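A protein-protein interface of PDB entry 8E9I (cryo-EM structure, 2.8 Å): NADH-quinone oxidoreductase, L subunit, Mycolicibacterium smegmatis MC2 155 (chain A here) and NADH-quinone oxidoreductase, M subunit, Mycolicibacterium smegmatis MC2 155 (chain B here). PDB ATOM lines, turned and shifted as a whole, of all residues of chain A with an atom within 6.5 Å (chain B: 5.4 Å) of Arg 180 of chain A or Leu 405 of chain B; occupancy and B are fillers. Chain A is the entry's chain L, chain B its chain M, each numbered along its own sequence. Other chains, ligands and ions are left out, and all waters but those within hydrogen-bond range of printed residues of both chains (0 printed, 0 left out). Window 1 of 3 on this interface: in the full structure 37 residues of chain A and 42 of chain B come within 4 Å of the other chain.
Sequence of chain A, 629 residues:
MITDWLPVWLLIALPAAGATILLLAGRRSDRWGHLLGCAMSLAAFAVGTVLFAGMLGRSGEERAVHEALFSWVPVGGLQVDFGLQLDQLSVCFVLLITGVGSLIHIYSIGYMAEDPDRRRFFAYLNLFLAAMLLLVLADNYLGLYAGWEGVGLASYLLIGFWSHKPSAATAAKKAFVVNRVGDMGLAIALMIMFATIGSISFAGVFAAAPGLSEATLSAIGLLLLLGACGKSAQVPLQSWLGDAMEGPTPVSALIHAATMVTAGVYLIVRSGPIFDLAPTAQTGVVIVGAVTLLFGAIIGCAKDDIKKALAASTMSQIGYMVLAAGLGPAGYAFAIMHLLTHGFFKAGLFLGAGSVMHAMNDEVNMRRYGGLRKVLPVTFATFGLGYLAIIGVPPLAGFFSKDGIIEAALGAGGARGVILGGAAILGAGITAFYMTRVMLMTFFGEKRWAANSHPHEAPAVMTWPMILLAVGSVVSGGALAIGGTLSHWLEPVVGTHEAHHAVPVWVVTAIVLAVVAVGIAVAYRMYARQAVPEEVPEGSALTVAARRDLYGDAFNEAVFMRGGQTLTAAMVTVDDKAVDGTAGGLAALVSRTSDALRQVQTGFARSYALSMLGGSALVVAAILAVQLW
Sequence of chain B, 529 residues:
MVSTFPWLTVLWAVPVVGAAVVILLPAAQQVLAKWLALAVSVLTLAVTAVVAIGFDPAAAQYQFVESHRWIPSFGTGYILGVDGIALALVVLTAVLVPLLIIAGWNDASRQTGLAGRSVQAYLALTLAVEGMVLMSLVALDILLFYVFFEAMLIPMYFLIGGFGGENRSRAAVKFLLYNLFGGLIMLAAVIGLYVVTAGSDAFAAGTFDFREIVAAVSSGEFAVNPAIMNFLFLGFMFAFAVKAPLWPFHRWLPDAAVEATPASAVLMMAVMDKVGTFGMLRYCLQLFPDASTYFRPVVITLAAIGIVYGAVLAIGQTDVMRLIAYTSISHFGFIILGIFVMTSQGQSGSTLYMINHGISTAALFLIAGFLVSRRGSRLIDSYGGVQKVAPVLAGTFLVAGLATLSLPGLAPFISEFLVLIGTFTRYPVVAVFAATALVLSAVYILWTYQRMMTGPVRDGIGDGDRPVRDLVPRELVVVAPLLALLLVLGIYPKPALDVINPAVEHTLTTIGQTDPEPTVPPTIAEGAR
Among the printed residues, merely in contact across the chains: Tyr 145 of chain A with Pro 408 of chain B (3.9 Å), Glu 149 of chain A with Leu 407 of chain B (3.9 Å), Glu 149 of chain A with Pro 408 of chain B (3.1 Å), Phe 176 of chain A with Leu 405 of chain B (3.7 Å), Phe 176 of chain A with Leu 446 of chain B (3.2 Å), Arg 180 of chain A with Leu 438 of chain B (3.3 Å), Arg 180 of chain A with Val 439 of chain B (3.7 Å), Arg 180 of chain A with Ala 442 of chain B (3.7 Å) and Val 181 of chain A with Val 439 of chain B (3.8 Å).
Of the 13 printed residues of chain A, 5 touch a printed residue of chain B.
Printed residues of chain A that touch a printed residue of chain B: Tyr 145, Glu 149, Phe 176, Arg 180 and Val 181.
Hydrophobic or aromatic side chains of chain A within 4 Å of the printed part of chain B: Tyr 145 and Phe 176.
Of the 16 printed residues of chain B, 8 touch a printed residue of chain A.
Hydrophobic or aromatic side chains of chain B within 4 Å of the printed part of chain A: Leu 405, Leu 407, Pro 408, Val 439, Ala 442 and Leu 446.
Among the printed residues, no Asp or Glu carboxylate lies within 4 Å of a Lys or Arg side-chain nitrogen of the other chain.
Of chain B, only Leu 405, Ser 406, Leu 438, Val 439 and Ala 442 come within 4 Å of Arg 180 of chain A.
Of chain A, only Phe 176 and Arg 180 come within 4 Å of Leu 405 of chain B.
Of the printed residues of chain B, Glu 149 of chain A touches Leu 407 (3.9 Å) and Pro 408 (3.1 Å).
Of the printed residues of chain B, Tyr 145 of chain A touches Pro 408.
Printed residues of chain A within 4 Å of Val 439 of chain B: Arg 180 and Val 181.
Of the printed residues of chain A, Pro 408 of chain B touches Tyr 145 (3.9 Å) and Glu 149 (3.1 Å).
Of the printed residues of chain B, Phe 176 of chain A touches Leu 405 (3.7 Å) and Leu 446 (3.2 Å).
Val 177 of chain A touches none of the printed residues of chain B.
Ser 441 of chain B touches none of the printed residues of chain A.
The nearest printed residue of chain A that does not touch Pro 408 of chain B is Arg 180 of chain A (4.8 Å).
The backbone carbonyl oxygen (O) of Asp 183 of chain A is in hydrogen-bond range of the side-chain hydroxyl (OH) of Tyr 145 of chain A, 3.1 Å away.
The backbone carbonyl oxygen of Leu 402 of chain B lies within hydrogen-bond range of the backbone NH of Leu 407 of chain B, at 3.3 Å.
The side-chain hydroxyl (OG) of Ser 441 of chain B is in hydrogen-bond range of the backbone carbonyl oxygen (O) of Leu 438 of chain B.
The backbone carbonyl oxygen (O) of Leu 405 of chain B sits at hydrogen-bond distance from the guanidinium group (NH2) of Arg 180 of chain A (3.0 Å).
The backbone carbonyl oxygen of Ser 406 of chain B lies within hydrogen-bond range of the guanidinium group of Arg 180 of chain A.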
ATOM      1  N   TYR A 145       5.789  27.501  20.140  1.00  0.00           N
ATOM      2  CA  TYR A 145       4.364  27.245  19.964  1.00  0.00           C
ATOM      3  C   TYR A 145       3.856  26.248  20.992  1.00  0.00           C
ATOM      4  O   TYR A 145       2.728  26.366  21.484  1.00  0.00           O
ATOM      5  CB  TYR A 145       4.085  26.733  18.550  1.00  0.00           C
ATOM      6  CG  TYR A 145       2.626  26.796  18.187  1.00  0.00           C
ATOM      7  CD1 TYR A 145       2.085  27.931  17.613  1.00  0.00           C
ATOM      8  CD2 TYR A 145       1.784  25.725  18.434  1.00  0.00           C
ATOM      9  CE1 TYR A 145       0.748  27.998  17.292  1.00  0.00           C
ATOM     10  CE2 TYR A 145       0.448  25.782  18.116  1.00  0.00           C
ATOM     11  CZ  TYR A 145      -0.066  26.921  17.546  1.00  0.00           C
ATOM     12  OH  TYR A 145      -1.398  26.983  17.223  1.00  0.00           O
ATOM     13  N   GLU A 149       0.781  27.257  23.444  1.00  0.00           N
ATOM     14  CA  GLU A 149      -0.463  26.534  23.648  1.00  0.00           C
ATOM     15  C   GLU A 149      -0.552  25.976  25.061  1.00  0.00           C
ATOM     16  O   GLU A 149      -1.649  25.872  25.618  1.00  0.00           O
ATOM     17  CB  GLU A 149      -0.590  25.415  22.619  1.00  0.00           C
ATOM     18  N   ALA A 175     -11.538  33.003  26.792  1.00  0.00           N
ATOM     19  CA  ALA A 175     -10.110  33.272  26.825  1.00  0.00           C
ATOM     20  C   ALA A 175      -9.358  32.283  25.955  1.00  0.00           C
ATOM     21  O   ALA A 175      -8.510  32.671  25.144  1.00  0.00           O
ATOM     22  CB  ALA A 175      -9.600  33.215  28.264  1.00  0.00           C
ATOM     23  N   PHE A 176      -9.667  30.994  26.094  1.00  0.00           N
ATOM     24  CA  PHE A 176      -8.935  29.999  25.327  1.00  0.00           C
ATOM     25  C   PHE A 176      -9.216  30.133  23.841  1.00  0.00           C
ATOM     26  O   PHE A 176      -8.324  29.924  23.023  1.00  0.00           O
ATOM     27  CB  PHE A 176      -9.273  28.589  25.793  1.00  0.00           C
ATOM     28  CG  PHE A 176      -8.348  27.544  25.239  1.00  0.00           C
ATOM     29  CD1 PHE A 176      -8.520  27.063  23.956  1.00  0.00           C
ATOM     30  CD2 PHE A 176      -7.301  27.061  25.994  1.00  0.00           C
ATOM     31  CE1 PHE A 176      -7.673  26.111  23.441  1.00  0.00           C
ATOM     32  CE2 PHE A 176      -6.447  26.106  25.482  1.00  0.00           C
ATOM     33  CZ  PHE A 176      -6.634  25.630  24.205  1.00  0.00           C
ATOM     34  N   VAL A 177     -10.447  30.467  23.463  1.00  0.00           N
ATOM     35  CA  VAL A 177     -10.778  30.546  22.043  1.00  0.00           C
ATOM     36  C   VAL A 177     -10.100  31.754  21.406  1.00  0.00           C
ATOM     37  O   VAL A 177      -9.607  31.685  20.275  1.00  0.00           O
ATOM     38  CB  VAL A 177     -12.302  30.580  21.845  1.00  0.00           C
ATOM     39  CG1 VAL A 177     -12.634  30.842  20.386  1.00  0.00           C
ATOM     40  CG2 VAL A 177     -12.919  29.273  22.308  1.00  0.00           C
ATOM     41  N   VAL A 178     -10.075  32.883  22.113  1.00  0.00           N
ATOM     42  CA  VAL A 178      -9.339  34.030  21.590  1.00  0.00           C
ATOM     43  C   VAL A 178      -7.850  33.714  21.517  1.00  0.00           C
ATOM     44  O   VAL A 178      -7.177  34.038  20.525  1.00  0.00           O
ATOM     45  CB  VAL A 178      -9.617  35.275  22.449  1.00  0.00           C
ATOM     46  CG1 VAL A 178      -8.765  36.433  21.990  1.00  0.00           C
ATOM     47  CG2 VAL A 178     -11.088  35.644  22.369  1.00  0.00           C
ATOM     48  N   ASN A 179      -7.308  33.073  22.548  1.00  0.00           N
ATOM     49  CA  ASN A 179      -5.920  32.647  22.494  1.00  0.00           C
ATOM     50  C   ASN A 179      -5.700  31.670  21.347  1.00  0.00           C
ATOM     51  O   ASN A 179      -4.605  31.586  20.793  1.00  0.00           O
ATOM     52  CB  ASN A 179      -5.525  32.021  23.829  1.00  0.00           C
ATOM     53  CG  ASN A 179      -4.113  32.352  24.236  1.00  0.00           C
ATOM     54  OD1 ASN A 179      -3.336  32.898  23.453  1.00  0.00           O
ATOM     55  ND2 ASN A 179      -3.776  32.047  25.480  1.00  0.00           N
ATOM     56  N   ARG A 180      -6.740  30.927  20.969  1.00  0.00           N
ATOM     57  CA  ARG A 180      -6.612  29.972  19.874  1.00  0.00           C
ATOM     58  C   ARG A 180      -6.628  30.683  18.532  1.00  0.00           C
ATOM     59  O   ARG A 180      -6.000  30.234  17.571  1.00  0.00           O
ATOM     60  CB  ARG A 180      -7.735  28.938  19.944  1.00  0.00           C
ATOM     61  CG  ARG A 180      -7.411  27.600  19.290  1.00  0.00           C
ATOM     62  CD  ARG A 180      -6.189  26.940  19.903  1.00  0.00           C
ATOM     63  NE  ARG A 180      -5.929  25.628  19.327  1.00  0.00           N
ATOM     64  CZ  ARG A 180      -4.788  24.966  19.465  1.00  0.00           C
ATOM     65  NH1 ARG A 180      -3.779  25.465  20.161  1.00  0.00           N
ATOM     66  NH2 ARG A 180      -4.655  23.776  18.887  1.00  0.00           N
ATOM     67  N   VAL A 181      -7.368  31.784  18.441  1.00  0.00           N
ATOM     68  CA  VAL A 181      -7.253  32.650  17.270  1.00  0.00           C
ATOM     69  C   VAL A 181      -5.823  33.149  17.147  1.00  0.00           C
ATOM     70  O   VAL A 181      -5.217  33.133  16.065  1.00  0.00           O
ATOM     71  CB  VAL A 181      -8.243  33.822  17.366  1.00  0.00           C
ATOM     72  CG1 VAL A 181      -7.982  34.817  16.251  1.00  0.00           C
ATOM     73  CG2 VAL A 181      -9.663  33.309  17.312  1.00  0.00           C
ATOM     74  N   GLY A 182      -5.261  33.600  18.266  1.00  0.00           N
ATOM     75  CA  GLY A 182      -3.857  33.976  18.266  1.00  0.00           C
ATOM     76  C   GLY A 182      -2.960  32.823  17.856  1.00  0.00           C
ATOM     77  O   GLY A 182      -1.976  33.009  17.137  1.00  0.00           O
ATOM     78  N   ASP A 183      -3.294  31.619  18.313  1.00  0.00           N
ATOM     79  CA  ASP A 183      -2.524  30.433  17.968  1.00  0.00           C
ATOM     80  C   ASP A 183      -2.585  30.143  16.479  1.00  0.00           C
ATOM     81  O   ASP A 183      -1.582  29.747  15.886  1.00  0.00           O
ATOM     82  CB  ASP A 183      -3.041  29.233  18.758  1.00  0.00           C
ATOM     83  N   MET A 184      -3.752  30.320  15.867  1.00  0.00           N
ATOM     84  CA  MET A 184      -3.863  30.162  14.422  1.00  0.00           C
ATOM     85  C   MET A 184      -2.998  31.188  13.710  1.00  0.00           C
ATOM     86  O   MET A 184      -2.321  30.874  12.727  1.00  0.00           O
ATOM     87  CB  MET A 184      -5.323  30.291  13.989  1.00  0.00           C
ATOM     88  N   GLY A 185      -3.013  32.428  14.193  1.00  0.00           N
ATOM     89  CA  GLY A 185      -2.133  33.431  13.612  1.00  0.00           C
ATOM     90  C   GLY A 185      -0.678  33.014  13.679  1.00  0.00           C
ATOM     91  O   GLY A 185       0.061  33.098  12.694  1.00  0.00           O
ATOM     92  N   HIS B 331     -11.046  15.529  11.142  1.00  0.00           N
ATOM     93  CA  HIS B 331      -9.707  14.963  11.228  1.00  0.00           C
ATOM     94  C   HIS B 331      -9.374  14.110  10.010  1.00  0.00           C
ATOM     95  O   HIS B 331      -8.217  14.079   9.575  1.00  0.00           O
ATOM     96  CB  HIS B 331      -9.573  14.163  12.517  1.00  0.00           C
ATOM     97  CG  HIS B 331      -9.688  15.006  13.745  1.00  0.00           C
ATOM     98  ND1 HIS B 331      -9.248  16.312  13.786  1.00  0.00           N
ATOM     99  CD2 HIS B 331     -10.184  14.738  14.975  1.00  0.00           C
ATOM    100  CE1 HIS B 331      -9.469  16.812  14.988  1.00  0.00           C
ATOM    101  NE2 HIS B 331     -10.037  15.876  15.729  1.00  0.00           N
ATOM    102  N   ALA B 400      -8.754  14.222  26.627  1.00  0.00           N
ATOM    103  CA  ALA B 400      -9.056  13.718  25.297  1.00  0.00           C
ATOM    104  C   ALA B 400      -9.444  14.844  24.356  1.00  0.00           C
ATOM    105  O   ALA B 400      -8.996  14.866  23.207  1.00  0.00           O
ATOM    106  CB  ALA B 400     -10.173  12.682  25.377  1.00  0.00           C
ATOM    107  N   GLY B 401     -10.267  15.780  24.816  1.00  0.00           N
ATOM    108  CA  GLY B 401     -10.663  16.899  23.988  1.00  0.00           C
ATOM    109  C   GLY B 401      -9.454  17.698  23.564  1.00  0.00           C
ATOM    110  O   GLY B 401      -9.298  18.041  22.390  1.00  0.00           O
ATOM    111  N   LEU B 402      -8.578  17.987  24.525  1.00  0.00           N
ATOM    112  CA  LEU B 402      -7.321  18.645  24.202  1.00  0.00           C
ATOM    113  C   LEU B 402      -6.576  17.890  23.114  1.00  0.00           C
ATOM    114  O   LEU B 402      -6.019  18.507  22.201  1.00  0.00           O
ATOM    115  CB  LEU B 402      -6.458  18.764  25.458  1.00  0.00           C
ATOM    116  CG  LEU B 402      -7.032  19.633  26.577  1.00  0.00           C
ATOM    117  CD1 LEU B 402      -6.108  19.637  27.777  1.00  0.00           C
ATOM    118  CD2 LEU B 402      -7.267  21.047  26.085  1.00  0.00           C
ATOM    119  N   ALA B 403      -6.558  16.561  23.191  1.00  0.00           N
ATOM    120  CA  ALA B 403      -5.912  15.783  22.142  1.00  0.00           C
ATOM    121  C   ALA B 403      -6.582  16.034  20.799  1.00  0.00           C
ATOM    122  O   ALA B 403      -5.930  16.434  19.829  1.00  0.00           O
ATOM    123  CB  ALA B 403      -5.945  14.296  22.494  1.00  0.00           C
ATOM    124  N   THR B 404      -7.899  15.841  20.733  1.00  0.00           N
ATOM    125  CA  THR B 404      -8.624  16.109  19.499  1.00  0.00           C
ATOM    126  C   THR B 404      -8.603  17.586  19.150  1.00  0.00           C
ATOM    127  O   THR B 404      -8.929  17.953  18.017  1.00  0.00           O
ATOM    128  CB  THR B 404     -10.070  15.625  19.615  1.00  0.00           C
ATOM    129  OG1 THR B 404     -10.667  16.181  20.790  1.00  0.00           O
ATOM    130  CG2 THR B 404     -10.127  14.106  19.695  1.00  0.00           C
ATOM    131  N   LEU B 405      -8.235  18.437  20.104  1.00  0.00           N
ATOM    132  CA  LEU B 405      -8.098  19.864  19.863  1.00  0.00           C
ATOM    133  C   LEU B 405      -6.751  20.226  19.252  1.00  0.00           C
ATOM    134  O   LEU B 405      -6.536  21.389  18.901  1.00  0.00           O
ATOM    135  CB  LEU B 405      -8.300  20.604  21.186  1.00  0.00           C
ATOM    136  CG  LEU B 405      -7.970  22.087  21.288  1.00  0.00           C
ATOM    137  CD1 LEU B 405      -8.733  22.874  20.260  1.00  0.00           C
ATOM    138  CD2 LEU B 405      -8.306  22.565  22.680  1.00  0.00           C
ATOM    139  N   SER B 406      -5.849  19.258  19.104  1.00  0.00           N
ATOM    140  CA  SER B 406      -4.516  19.490  18.554  1.00  0.00           C
ATOM    141  C   SER B 406      -3.725  20.460  19.438  1.00  0.00           C
ATOM    142  O   SER B 406      -3.261  21.517  19.006  1.00  0.00           O
ATOM    143  CB  SER B 406      -4.606  20.016  17.117  1.00  0.00           C
ATOM    144  OG  SER B 406      -5.261  19.089  16.274  1.00  0.00           O
ATOM    145  N   LEU B 407      -3.580  20.062  20.691  1.00  0.00           N
ATOM    146  CA  LEU B 407      -2.742  20.832  21.590  1.00  0.00           C
ATOM    147  C   LEU B 407      -1.342  20.227  21.656  1.00  0.00           C
ATOM    148  O   LEU B 407      -1.196  19.012  21.814  1.00  0.00           O
ATOM    149  CB  LEU B 407      -3.350  20.873  22.992  1.00  0.00           C
ATOM    150  CG  LEU B 407      -2.652  21.845  23.940  1.00  0.00           C
ATOM    151  CD1 LEU B 407      -3.671  22.650  24.719  1.00  0.00           C
ATOM    152  CD2 LEU B 407      -1.720  21.111  24.881  1.00  0.00           C
ATOM    153  N   PRO B 408      -0.284  21.034  21.538  1.00  0.00           N
ATOM    154  CA  PRO B 408       1.064  20.455  21.430  1.00  0.00           C
ATOM    155  C   PRO B 408       1.435  19.526  22.568  1.00  0.00           C
ATOM    156  O   PRO B 408       2.103  18.515  22.321  1.00  0.00           O
ATOM    157  CB  PRO B 408       1.972  21.690  21.401  1.00  0.00           C
ATOM    158  CG  PRO B 408       1.105  22.770  20.884  1.00  0.00           C
ATOM    159  CD  PRO B 408      -0.235  22.503  21.475  1.00  0.00           C
ATOM    160  N   LEU B 438      -8.076  24.945  13.772  1.00  0.00           N
ATOM    161  CA  LEU B 438      -7.529  25.020  15.122  1.00  0.00           C
ATOM    162  C   LEU B 438      -8.478  25.785  16.036  1.00  0.00           C
ATOM    163  O   LEU B 438      -8.716  25.394  17.184  1.00  0.00           O
ATOM    164  CB  LEU B 438      -6.150  25.678  15.096  1.00  0.00           C
ATOM    165  N   VAL B 439      -9.032  26.887  15.530  1.00  0.00           N
ATOM    166  CA  VAL B 439     -10.029  27.643  16.277  1.00  0.00           C
ATOM    167  C   VAL B 439     -11.315  26.838  16.409  1.00  0.00           C
ATOM    168  O   VAL B 439     -11.920  26.756  17.488  1.00  0.00           O
ATOM    169  CB  VAL B 439     -10.286  28.995  15.587  1.00  0.00           C
ATOM    170  CG1 VAL B 439     -11.348  29.776  16.326  1.00  0.00           C
ATOM    171  CG2 VAL B 439      -8.999  29.794  15.488  1.00  0.00           C
ATOM    172  N   SER B 441     -11.861  23.688  16.394  1.00  0.00           N
ATOM    173  CA  SER B 441     -11.708  22.594  17.339  1.00  0.00           C
ATOM    174  C   SER B 441     -11.834  23.081  18.767  1.00  0.00           C
ATOM    175  O   SER B 441     -12.559  22.473  19.563  1.00  0.00           O
ATOM    176  CB  SER B 441     -10.363  21.907  17.118  1.00  0.00           C
ATOM    177  OG  SER B 441      -9.296  22.832  17.211  1.00  0.00           O
ATOM    178  N   ALA B 442     -11.145  24.168  19.111  1.00  0.00           N
ATOM    179  CA  ALA B 442     -11.340  24.751  20.427  1.00  0.00           C
ATOM    180  C   ALA B 442     -12.814  24.999  20.674  1.00  0.00           C
ATOM    181  O   ALA B 442     -13.338  24.676  21.744  1.00  0.00           O
ATOM    182  CB  ALA B 442     -10.545  26.049  20.553  1.00  0.00           C
ATOM    183  N   ILE B 445     -14.884  21.662  21.136  1.00  0.00           N
ATOM    184  CA  ILE B 445     -14.411  20.858  22.258  1.00  0.00           C
ATOM    185  C   ILE B 445     -14.723  21.552  23.575  1.00  0.00           C
ATOM    186  O   ILE B 445     -15.385  20.992  24.458  1.00  0.00           O
ATOM    187  CB  ILE B 445     -12.904  20.577  22.118  1.00  0.00           C
ATOM    188  CG1 ILE B 445     -12.626  19.698  20.893  1.00  0.00           C
ATOM    189  CG2 ILE B 445     -12.366  19.920  23.376  1.00  0.00           C
ATOM    190  CD1 ILE B 445     -13.287  18.335  20.922  1.00  0.00           C
ATOM    191  N   LEU B 446     -14.240  22.784  23.730  1.00  0.00           N
ATOM    192  CA  LEU B 446     -14.413  23.474  24.996  1.00  0.00           C
ATOM    193  C   LEU B 446     -15.865  23.836  25.244  1.00  0.00           C
ATOM    194  O   LEU B 446     -16.307  23.803  26.392  1.00  0.00           O
ATOM    195  CB  LEU B 446     -13.532  24.714  25.035  1.00  0.00           C
ATOM    196  CG  LEU B 446     -12.040  24.394  24.927  1.00  0.00           C
ATOM    197  CD1 LEU B 446     -11.231  25.670  24.874  1.00  0.00           C
ATOM    198  CD2 LEU B 446     -11.574  23.505  26.074  1.00  0.00           C
